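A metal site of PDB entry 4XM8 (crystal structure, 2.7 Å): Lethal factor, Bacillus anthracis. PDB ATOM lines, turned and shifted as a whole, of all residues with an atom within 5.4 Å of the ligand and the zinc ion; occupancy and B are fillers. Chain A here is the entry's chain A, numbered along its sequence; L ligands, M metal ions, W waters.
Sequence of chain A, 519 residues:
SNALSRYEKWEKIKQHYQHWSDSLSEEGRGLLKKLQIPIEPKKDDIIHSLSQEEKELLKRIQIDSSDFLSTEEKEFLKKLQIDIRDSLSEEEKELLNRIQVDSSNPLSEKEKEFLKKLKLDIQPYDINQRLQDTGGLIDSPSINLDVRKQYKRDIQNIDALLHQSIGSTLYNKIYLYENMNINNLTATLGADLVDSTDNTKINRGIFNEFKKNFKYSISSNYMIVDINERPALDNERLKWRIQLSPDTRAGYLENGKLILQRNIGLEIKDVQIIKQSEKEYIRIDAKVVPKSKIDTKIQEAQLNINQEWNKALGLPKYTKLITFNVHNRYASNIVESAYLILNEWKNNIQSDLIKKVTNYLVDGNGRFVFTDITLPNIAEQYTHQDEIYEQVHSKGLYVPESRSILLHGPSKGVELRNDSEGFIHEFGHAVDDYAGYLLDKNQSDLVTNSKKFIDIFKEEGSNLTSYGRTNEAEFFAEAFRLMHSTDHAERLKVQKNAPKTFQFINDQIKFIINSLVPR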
ATOM      1  N   THR A 188       7.172   1.471  17.385  1.00  0.00           N
ATOM      2  CA  THR A 188       6.296   2.120  18.348  1.00  0.00           C
ATOM      3  C   THR A 188       5.213   1.168  18.839  1.00  0.00           C
ATOM      4  O   THR A 188       4.981   1.047  20.046  1.00  0.00           O
ATOM      5  CB  THR A 188       5.638   3.381  17.746  1.00  0.00           C
ATOM      6  N   VAL A 392      21.501  13.573  10.088  1.00  0.00           N
ATOM      7  CA  VAL A 392      20.927  12.947  11.263  1.00  0.00           C
ATOM      8  C   VAL A 392      19.789  12.005  10.905  1.00  0.00           C
ATOM      9  O   VAL A 392      18.927  12.348  10.099  1.00  0.00           O
ATOM     10  CB  VAL A 392      20.414  13.997  12.270  1.00  0.00           C
ATOM     11  CG1 VAL A 392      19.881  13.329  13.516  1.00  0.00           C
ATOM     12  CG2 VAL A 392      21.511  14.991  12.628  1.00  0.00           C
ATOM     13  N   SER A 394      16.712  10.046  12.962  1.00  0.00           N
ATOM     14  CA  SER A 394      15.997   9.974  14.222  1.00  0.00           C
ATOM     15  C   SER A 394      14.524   9.843  13.902  1.00  0.00           C
ATOM     16  O   SER A 394      14.154   9.718  12.738  1.00  0.00           O
ATOM     17  CB  SER A 394      16.267  11.208  15.092  1.00  0.00           C
ATOM     18  OG  SER A 394      15.874  12.396  14.441  1.00  0.00           O
ATOM     19  N   LYS A 395      13.669   9.875  14.920  1.00  0.00           N
ATOM     20  CA  LYS A 395      12.246   9.731  14.691  1.00  0.00           C
ATOM     21  C   LYS A 395      11.676  10.989  14.066  1.00  0.00           C
ATOM     22  O   LYS A 395      10.808  10.937  13.204  1.00  0.00           O
ATOM     23  CB  LYS A 395      11.516   9.401  15.996  1.00  0.00           C
ATOM     24  CG  LYS A 395      10.027   9.150  15.827  1.00  0.00           C
ATOM     25  CD  LYS A 395       9.686   7.709  16.100  1.00  0.00           C
ATOM     26  CE  LYS A 395       8.229   7.416  15.774  1.00  0.00           C
ATOM     27  NZ  LYS A 395       7.912   7.657  14.346  1.00  0.00           N
ATOM     28  N   GLY A 396      12.192  12.133  14.515  1.00  0.00           N
ATOM     29  CA  GLY A 396      11.680  13.410  14.078  1.00  0.00           C
ATOM     30  C   GLY A 396      12.772  14.466  14.004  1.00  0.00           C
ATOM     31  O   GLY A 396      13.847  14.304  14.570  1.00  0.00           O
ATOM     32  N   LEU A 397      12.482  15.554  13.302  1.00  0.00           N
ATOM     33  CA  LEU A 397      13.470  16.591  13.073  1.00  0.00           C
ATOM     34  C   LEU A 397      12.797  17.881  12.620  1.00  0.00           C
ATOM     35  O   LEU A 397      11.750  17.845  11.982  1.00  0.00           O
ATOM     36  CB  LEU A 397      14.492  16.132  12.043  1.00  0.00           C
ATOM     37  CG  LEU A 397      15.930  16.633  12.168  1.00  0.00           C
ATOM     38  CD1 LEU A 397      16.586  16.042  13.399  1.00  0.00           C
ATOM     39  CD2 LEU A 397      16.725  16.302  10.912  1.00  0.00           C
ATOM     40  N   TYR A 398      13.394  19.006  12.965  1.00  0.00           N
ATOM     41  CA  TYR A 398      12.999  20.281  12.363  1.00  0.00           C
ATOM     42  C   TYR A 398      14.193  20.902  11.660  1.00  0.00           C
ATOM     43  O   TYR A 398      15.261  21.083  12.252  1.00  0.00           O
ATOM     44  CB  TYR A 398      12.441  21.247  13.400  1.00  0.00           C
ATOM     45  CG  TYR A 398      12.101  22.586  12.779  1.00  0.00           C
ATOM     46  CD1 TYR A 398      10.982  22.730  11.969  1.00  0.00           C
ATOM     47  CD2 TYR A 398      12.916  23.696  12.987  1.00  0.00           C
ATOM     48  CE1 TYR A 398      10.673  23.939  11.395  1.00  0.00           C
ATOM     49  CE2 TYR A 398      12.622  24.906  12.404  1.00  0.00           C
ATOM     50  CZ  TYR A 398      11.498  25.028  11.614  1.00  0.00           C
ATOM     51  OH  TYR A 398      11.185  26.236  11.022  1.00  0.00           O
ATOM     52  N   LEU A 407       9.097  13.497   9.997  1.00  0.00           N
ATOM     53  CA  LEU A 407       8.730  12.475  10.962  1.00  0.00           C
ATOM     54  C   LEU A 407       8.894  11.079  10.384  1.00  0.00           C
ATOM     55  O   LEU A 407       8.250  10.727   9.392  1.00  0.00           O
ATOM     56  CB  LEU A 407       7.292  12.665  11.428  1.00  0.00           C
ATOM     57  CG  LEU A 407       6.997  12.082  12.806  1.00  0.00           C
ATOM     58  CD1 LEU A 407       7.695  12.900  13.871  1.00  0.00           C
ATOM     59  CD2 LEU A 407       5.501  12.024  13.059  1.00  0.00           C
ATOM     60  N   LYS A 412      11.831   3.840  16.679  1.00  0.00           N
ATOM     61  CA  LYS A 412      11.404   4.088  18.055  1.00  0.00           C
ATOM     62  C   LYS A 412      12.005   5.395  18.556  1.00  0.00           C
ATOM     63  O   LYS A 412      13.186   5.682  18.312  1.00  0.00           O
ATOM     64  CB  LYS A 412      11.805   2.935  18.974  1.00  0.00           C
ATOM     65  N   GLY A 413      11.211   6.186  19.259  1.00  0.00           N
ATOM     66  CA  GLY A 413      11.660   7.485  19.708  1.00  0.00           C
ATOM     67  C   GLY A 413      12.143   7.503  21.149  1.00  0.00           C
ATOM     68  O   GLY A 413      11.747   6.681  21.963  1.00  0.00           O
ATOM     69  N   VAL A 414      13.011   8.472  21.460  1.00  0.00           N
ATOM     70  CA  VAL A 414      13.569   8.605  22.792  1.00  0.00           C
ATOM     71  C   VAL A 414      12.571   9.216  23.769  1.00  0.00           C
ATOM     72  O   VAL A 414      12.098  10.339  23.567  1.00  0.00           O
ATOM     73  CB  VAL A 414      14.852   9.460  22.778  1.00  0.00           C
ATOM     74  CG1 VAL A 414      15.247   9.851  24.195  1.00  0.00           C
ATOM     75  CG2 VAL A 414      15.979   8.722  22.077  1.00  0.00           C
ATOM     76  N   LEU A 416       9.625   9.374  24.406  1.00  0.00           N
ATOM     77  CA  LEU A 416       8.270   9.773  24.067  1.00  0.00           C
ATOM     78  C   LEU A 416       7.366   8.559  23.870  1.00  0.00           C
ATOM     79  O   LEU A 416       7.829   7.473  23.536  1.00  0.00           O
ATOM     80  CB  LEU A 416       8.253  10.636  22.803  1.00  0.00           C
ATOM     81  CG  LEU A 416       9.010  11.963  22.871  1.00  0.00           C
ATOM     82  CD1 LEU A 416       8.696  12.822  21.655  1.00  0.00           C
ATOM     83  CD2 LEU A 416       8.665  12.684  24.155  1.00  0.00           C
ATOM     84  N   ARG A 417       6.061   8.769  24.078  1.00  0.00           N
ATOM     85  CA  ARG A 417       5.087   7.697  23.941  1.00  0.00           C
ATOM     86  C   ARG A 417       4.687   7.497  22.475  1.00  0.00           C
ATOM     87  O   ARG A 417       5.126   6.544  21.826  1.00  0.00           O
ATOM     88  CB  ARG A 417       3.843   7.985  24.782  1.00  0.00           C
ATOM     89  N   ASN A 418       3.849   8.399  21.973  1.00  0.00           N
ATOM     90  CA  ASN A 418       3.370   8.304  20.600  1.00  0.00           C
ATOM     91  C   ASN A 418       4.006   9.351  19.692  1.00  0.00           C
ATOM     92  O   ASN A 418       4.799  10.176  20.142  1.00  0.00           O
ATOM     93  CB  ASN A 418       1.845   8.429  20.561  1.00  0.00           C
ATOM     94  CG  ASN A 418       1.345   9.674  21.272  1.00  0.00           C
ATOM     95  OD1 ASN A 418       1.823  10.784  21.024  1.00  0.00           O
ATOM     96  ND2 ASN A 418       0.376   9.502  22.169  1.00  0.00           N
ATOM     97  N   ASP A 419       3.652   9.311  18.414  1.00  0.00           N
ATOM     98  CA  ASP A 419       4.206  10.231  17.435  1.00  0.00           C
ATOM     99  C   ASP A 419       3.551  11.606  17.534  1.00  0.00           C
ATOM    100  O   ASP A 419       4.115  12.602  17.079  1.00  0.00           O
ATOM    101  CB  ASP A 419       4.047   9.679  16.014  1.00  0.00           C
ATOM    102  CG  ASP A 419       4.613   8.277  15.874  1.00  0.00           C
ATOM    103  OD1 ASP A 419       5.204   7.771  16.848  1.00  0.00           O
ATOM    104  OD2 ASP A 419       4.481   7.693  14.774  1.00  0.00           O
ATOM    105  N   GLY A 422       5.570  13.675  19.513  1.00  0.00           N
ATOM    106  CA  GLY A 422       6.777  13.932  18.748  1.00  0.00           C
ATOM    107  C   GLY A 422       6.624  15.112  17.808  1.00  0.00           C
ATOM    108  O   GLY A 422       7.507  15.967  17.726  1.00  0.00           O
ATOM    109  N   PHE A 423       5.494  15.163  17.105  1.00  0.00           N
ATOM    110  CA  PHE A 423       5.239  16.236  16.155  1.00  0.00           C
ATOM    111  C   PHE A 423       5.149  17.588  16.856  1.00  0.00           C
ATOM    112  O   PHE A 423       5.761  18.563  16.422  1.00  0.00           O
ATOM    113  CB  PHE A 423       3.942  15.977  15.382  1.00  0.00           C
ATOM    114  CG  PHE A 423       3.641  16.999  14.332  1.00  0.00           C
ATOM    115  CD1 PHE A 423       4.240  16.920  13.085  1.00  0.00           C
ATOM    116  CD2 PHE A 423       2.767  18.047  14.585  1.00  0.00           C
ATOM    117  CE1 PHE A 423       3.972  17.862  12.109  1.00  0.00           C
ATOM    118  CE2 PHE A 423       2.494  18.989  13.622  1.00  0.00           C
ATOM    119  CZ  PHE A 423       3.095  18.896  12.375  1.00  0.00           C
ATOM    120  N   HIS A 425       6.432  18.436  19.601  1.00  0.00           N
ATOM    121  CA  HIS A 425       7.806  18.769  19.977  1.00  0.00           C
ATOM    122  C   HIS A 425       8.524  19.436  18.812  1.00  0.00           C
ATOM    123  O   HIS A 425       9.181  20.465  18.979  1.00  0.00           O
ATOM    124  CB  HIS A 425       8.553  17.510  20.425  1.00  0.00           C
ATOM    125  CG  HIS A 425      10.038  17.688  20.528  1.00  0.00           C
ATOM    126  ND1 HIS A 425      10.689  17.796  21.737  1.00  0.00           N
ATOM    127  CD2 HIS A 425      10.993  17.757  19.574  1.00  0.00           C
ATOM    128  CE1 HIS A 425      11.980  17.927  21.520  1.00  0.00           C
ATOM    129  NE2 HIS A 425      12.194  17.915  20.223  1.00  0.00           N
ATOM    130  N   GLU A 426       8.399  18.851  17.621  1.00  0.00           N
ATOM    131  CA  GLU A 426       9.001  19.423  16.425  1.00  0.00           C
ATOM    132  C   GLU A 426       8.423  20.786  16.109  1.00  0.00           C
ATOM    133  O   GLU A 426       9.120  21.694  15.655  1.00  0.00           O
ATOM    134  CB  GLU A 426       8.823  18.495  15.220  1.00  0.00           C
ATOM    135  CG  GLU A 426       9.327  17.077  15.424  1.00  0.00           C
ATOM    136  CD  GLU A 426      10.814  17.001  15.656  1.00  0.00           C
ATOM    137  OE1 GLU A 426      11.288  15.948  16.131  1.00  0.00           O
ATOM    138  OE2 GLU A 426      11.518  17.984  15.363  1.00  0.00           O
ATOM    139  N   HIS A 429       9.947  23.589  17.862  1.00  0.00           N
ATOM    140  CA  HIS A 429      11.149  24.068  17.187  1.00  0.00           C
ATOM    141  C   HIS A 429      10.820  25.158  16.174  1.00  0.00           C
ATOM    142  O   HIS A 429      11.569  26.130  16.031  1.00  0.00           O
ATOM    143  CB  HIS A 429      11.870  22.918  16.492  1.00  0.00           C
ATOM    144  CG  HIS A 429      12.855  22.208  17.368  1.00  0.00           C
ATOM    145  ND1 HIS A 429      13.588  22.858  18.333  1.00  0.00           N
ATOM    146  CD2 HIS A 429      13.220  20.910  17.422  1.00  0.00           C
ATOM    147  CE1 HIS A 429      14.373  21.986  18.944  1.00  0.00           C
ATOM    148  NE2 HIS A 429      14.166  20.797  18.412  1.00  0.00           N
ATOM    149  N   TYR A 467      16.155  14.389  27.980  1.00  0.00           N
ATOM    150  CA  TYR A 467      16.632  14.855  26.677  1.00  0.00           C
ATOM    151  C   TYR A 467      16.565  16.365  26.576  1.00  0.00           C
ATOM    152  O   TYR A 467      17.254  16.978  25.767  1.00  0.00           O
ATOM    153  CB  TYR A 467      15.831  14.214  25.536  1.00  0.00           C
ATOM    154  CG  TYR A 467      16.407  14.551  24.179  1.00  0.00           C
ATOM    155  CD1 TYR A 467      17.532  13.896  23.704  1.00  0.00           C
ATOM    156  CD2 TYR A 467      15.856  15.551  23.398  1.00  0.00           C
ATOM    157  CE1 TYR A 467      18.074  14.210  22.479  1.00  0.00           C
ATOM    158  CE2 TYR A 467      16.397  15.878  22.172  1.00  0.00           C
ATOM    159  CZ  TYR A 467      17.507  15.201  21.713  1.00  0.00           C
ATOM    160  OH  TYR A 467      18.048  15.528  20.487  1.00  0.00           O
ATOM    161  N   GLU A 474      16.584  22.234  22.382  1.00  0.00           N
ATOM    162  CA  GLU A 474      15.920  21.009  22.815  1.00  0.00           C
ATOM    163  C   GLU A 474      15.086  21.228  24.072  1.00  0.00           C
ATOM    164  O   GLU A 474      13.964  20.733  24.178  1.00  0.00           O
ATOM    165  CB  GLU A 474      16.944  19.899  23.065  1.00  0.00           C
ATOM    166  CG  GLU A 474      17.797  19.556  21.857  1.00  0.00           C
ATOM    167  CD  GLU A 474      16.975  18.976  20.717  1.00  0.00           C
ATOM    168  OE1 GLU A 474      15.813  18.621  20.965  1.00  0.00           O
ATOM    169  OE2 GLU A 474      17.503  18.882  19.585  1.00  0.00           O
ATOM    170  N   ALA A 477      11.919  22.979  23.192  1.00  0.00           N
ATOM    171  CA  ALA A 477      10.996  22.088  22.482  1.00  0.00           C
ATOM    172  C   ALA A 477      10.291  21.132  23.440  1.00  0.00           C
ATOM    173  O   ALA A 477       9.073  20.963  23.378  1.00  0.00           O
ATOM    174  CB  ALA A 477      11.731  21.317  21.406  1.00  0.00           C
ATOM    175  N   GLU A 478      11.060  20.514  24.325  1.00  0.00           N
ATOM    176  CA  GLU A 478      10.492  19.636  25.347  1.00  0.00           C
ATOM    177  C   GLU A 478       9.538  20.395  26.272  1.00  0.00           C
ATOM    178  O   GLU A 478       8.457  19.904  26.605  1.00  0.00           O
ATOM    179  CB  GLU A 478      11.594  18.970  26.167  1.00  0.00           C
ATOM    180  CG  GLU A 478      12.337  17.872  25.430  1.00  0.00           C
ATOM    181  CD  GLU A 478      11.474  16.641  25.196  1.00  0.00           C
ATOM    182  OE1 GLU A 478      11.641  15.652  25.941  1.00  0.00           O
ATOM    183  OE2 GLU A 478      10.635  16.671  24.265  1.00  0.00           O
HETATM  184  C1  LIG L   1      14.801  14.246  18.131  1.00  0.00           C
HETATM  185  C2  LIG L   1      14.461  15.708  18.264  1.00  0.00           C
HETATM  186  O1  LIG L   1      13.477  17.638  17.305  1.00  0.00           O
HETATM  187  N1  LIG L   1      14.110  13.335  19.067  1.00  0.00           N
HETATM  188  C3  LIG L   1      14.074  13.781  20.467  1.00  0.00           C
HETATM  189  C4  LIG L   1      12.664  13.627  21.032  1.00  0.00           C
HETATM  190  C5  LIG L   1      11.699  14.638  20.433  1.00  0.00           C
HETATM  191  C6  LIG L   1      12.646  13.714  22.558  1.00  0.00           C
HETATM  192  C7  LIG L   1      11.969  11.961  18.328  1.00  0.00           C
HETATM  193  C8  LIG L   1      11.217  11.000  18.996  1.00  0.00           C
HETATM  194  C9  LIG L   1       9.840  10.921  18.790  1.00  0.00           C
HETATM  195  C10 LIG L   1      11.359  12.844  17.446  1.00  0.00           C
HETATM  196  C11 LIG L   1       9.052   9.864  19.523  1.00  0.00           C
HETATM  197  C12 LIG L   1       7.607   8.024  19.257  1.00  0.00           C
HETATM  198  C13 LIG L   1      17.078  14.936  17.326  1.00  0.00           C
HETATM  199  O2  LIG L   1      14.970  16.495  19.391  1.00  0.00           O
HETATM  200  N2  LIG L   1      13.693  16.304  17.309  1.00  0.00           N
HETATM  201  S1  LIG L   1      13.547  11.998  18.589  1.00  0.00           S
HETATM  202  O3  LIG L   1      13.845  10.996  19.569  1.00  0.00           O
HETATM  203  O4  LIG L   1      14.180  11.638  17.361  1.00  0.00           O
HETATM  204  C14 LIG L   1       9.230  11.804  17.908  1.00  0.00           C
HETATM  205  C15 LIG L   1       9.982  12.764  17.241  1.00  0.00           C
HETATM  206  O5  LIG L   1       8.132   9.212  18.653  1.00  0.00           O
HETATM  207  C16 LIG L   1      16.306  14.152  18.378  1.00  0.00           C
HETATM  208  C17 LIG L   1      16.881  12.734  18.497  1.00  0.00           C
HETATM  209 ZN    ZN M   1      14.350  18.415  19.009  1.00  0.00          ZN
HETATM  210  O   HOH W   1      15.238  18.910  15.331  1.00  0.00           O
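Within 4 Å of the zinc ion: His 425, His 429 and Glu 474.
Along chain A the residues within 4 Å of the zinc ion span positions 425 to 474.
The nearest printed residue that does not touch the zinc ion is Tyr 467 (4.5 Å).
The zinc ion is bound by O2 of the ligand, O1 of the ligand, OE1 of Glu 474, NE2 of His 429 and NE2 of His 425.
O4 of the ligand sits at hydrogen-bond distance from N of Lys 395, 3.1 Å away.
An oxygen (O4) of the ligand lies close to the side-chain hydroxyl (OG) of Ser 394.
O2 of the ligand sits close to OH of Tyr 467 (3.4 Å).
The backbone carbonyl oxygen of Gly 396 sits at hydrogen-bond distance from a nitrogen (N2) of the ligand, at 3.4 Å.
The backbone NH (N) of Val 414 sits at hydrogen-bond distance from an oxygen (O3) of the ligand (3.3 Å).
The side-chain carboxylate of Glu 426 lies within hydrogen-bond range of a nitrogen (N2) of the ligand (2.7 Å).
Residues that only touch the ligand: Gly 413, Leu 416, Arg 417, Asn 418, Asp 419, Gly 422 and Glu 478.
NZ of Lys 395 lies within salt-bridge range of OD2 of Asp 419 (3.5 Å).
OE2 of Glu 426 is in hydrogen-bond range of N of Tyr 398 (3.2 Å).
ND1 of His 425 lies within hydrogen-bond range of OE2 of Glu 478 (2.8 Å).
O of Gly 396 sits at hydrogen-bond distance from OG of Ser 394.
The backbone NH of Leu 397 is in hydrogen-bond range of the side-chain carboxylate of Glu 426 (3.1 Å).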
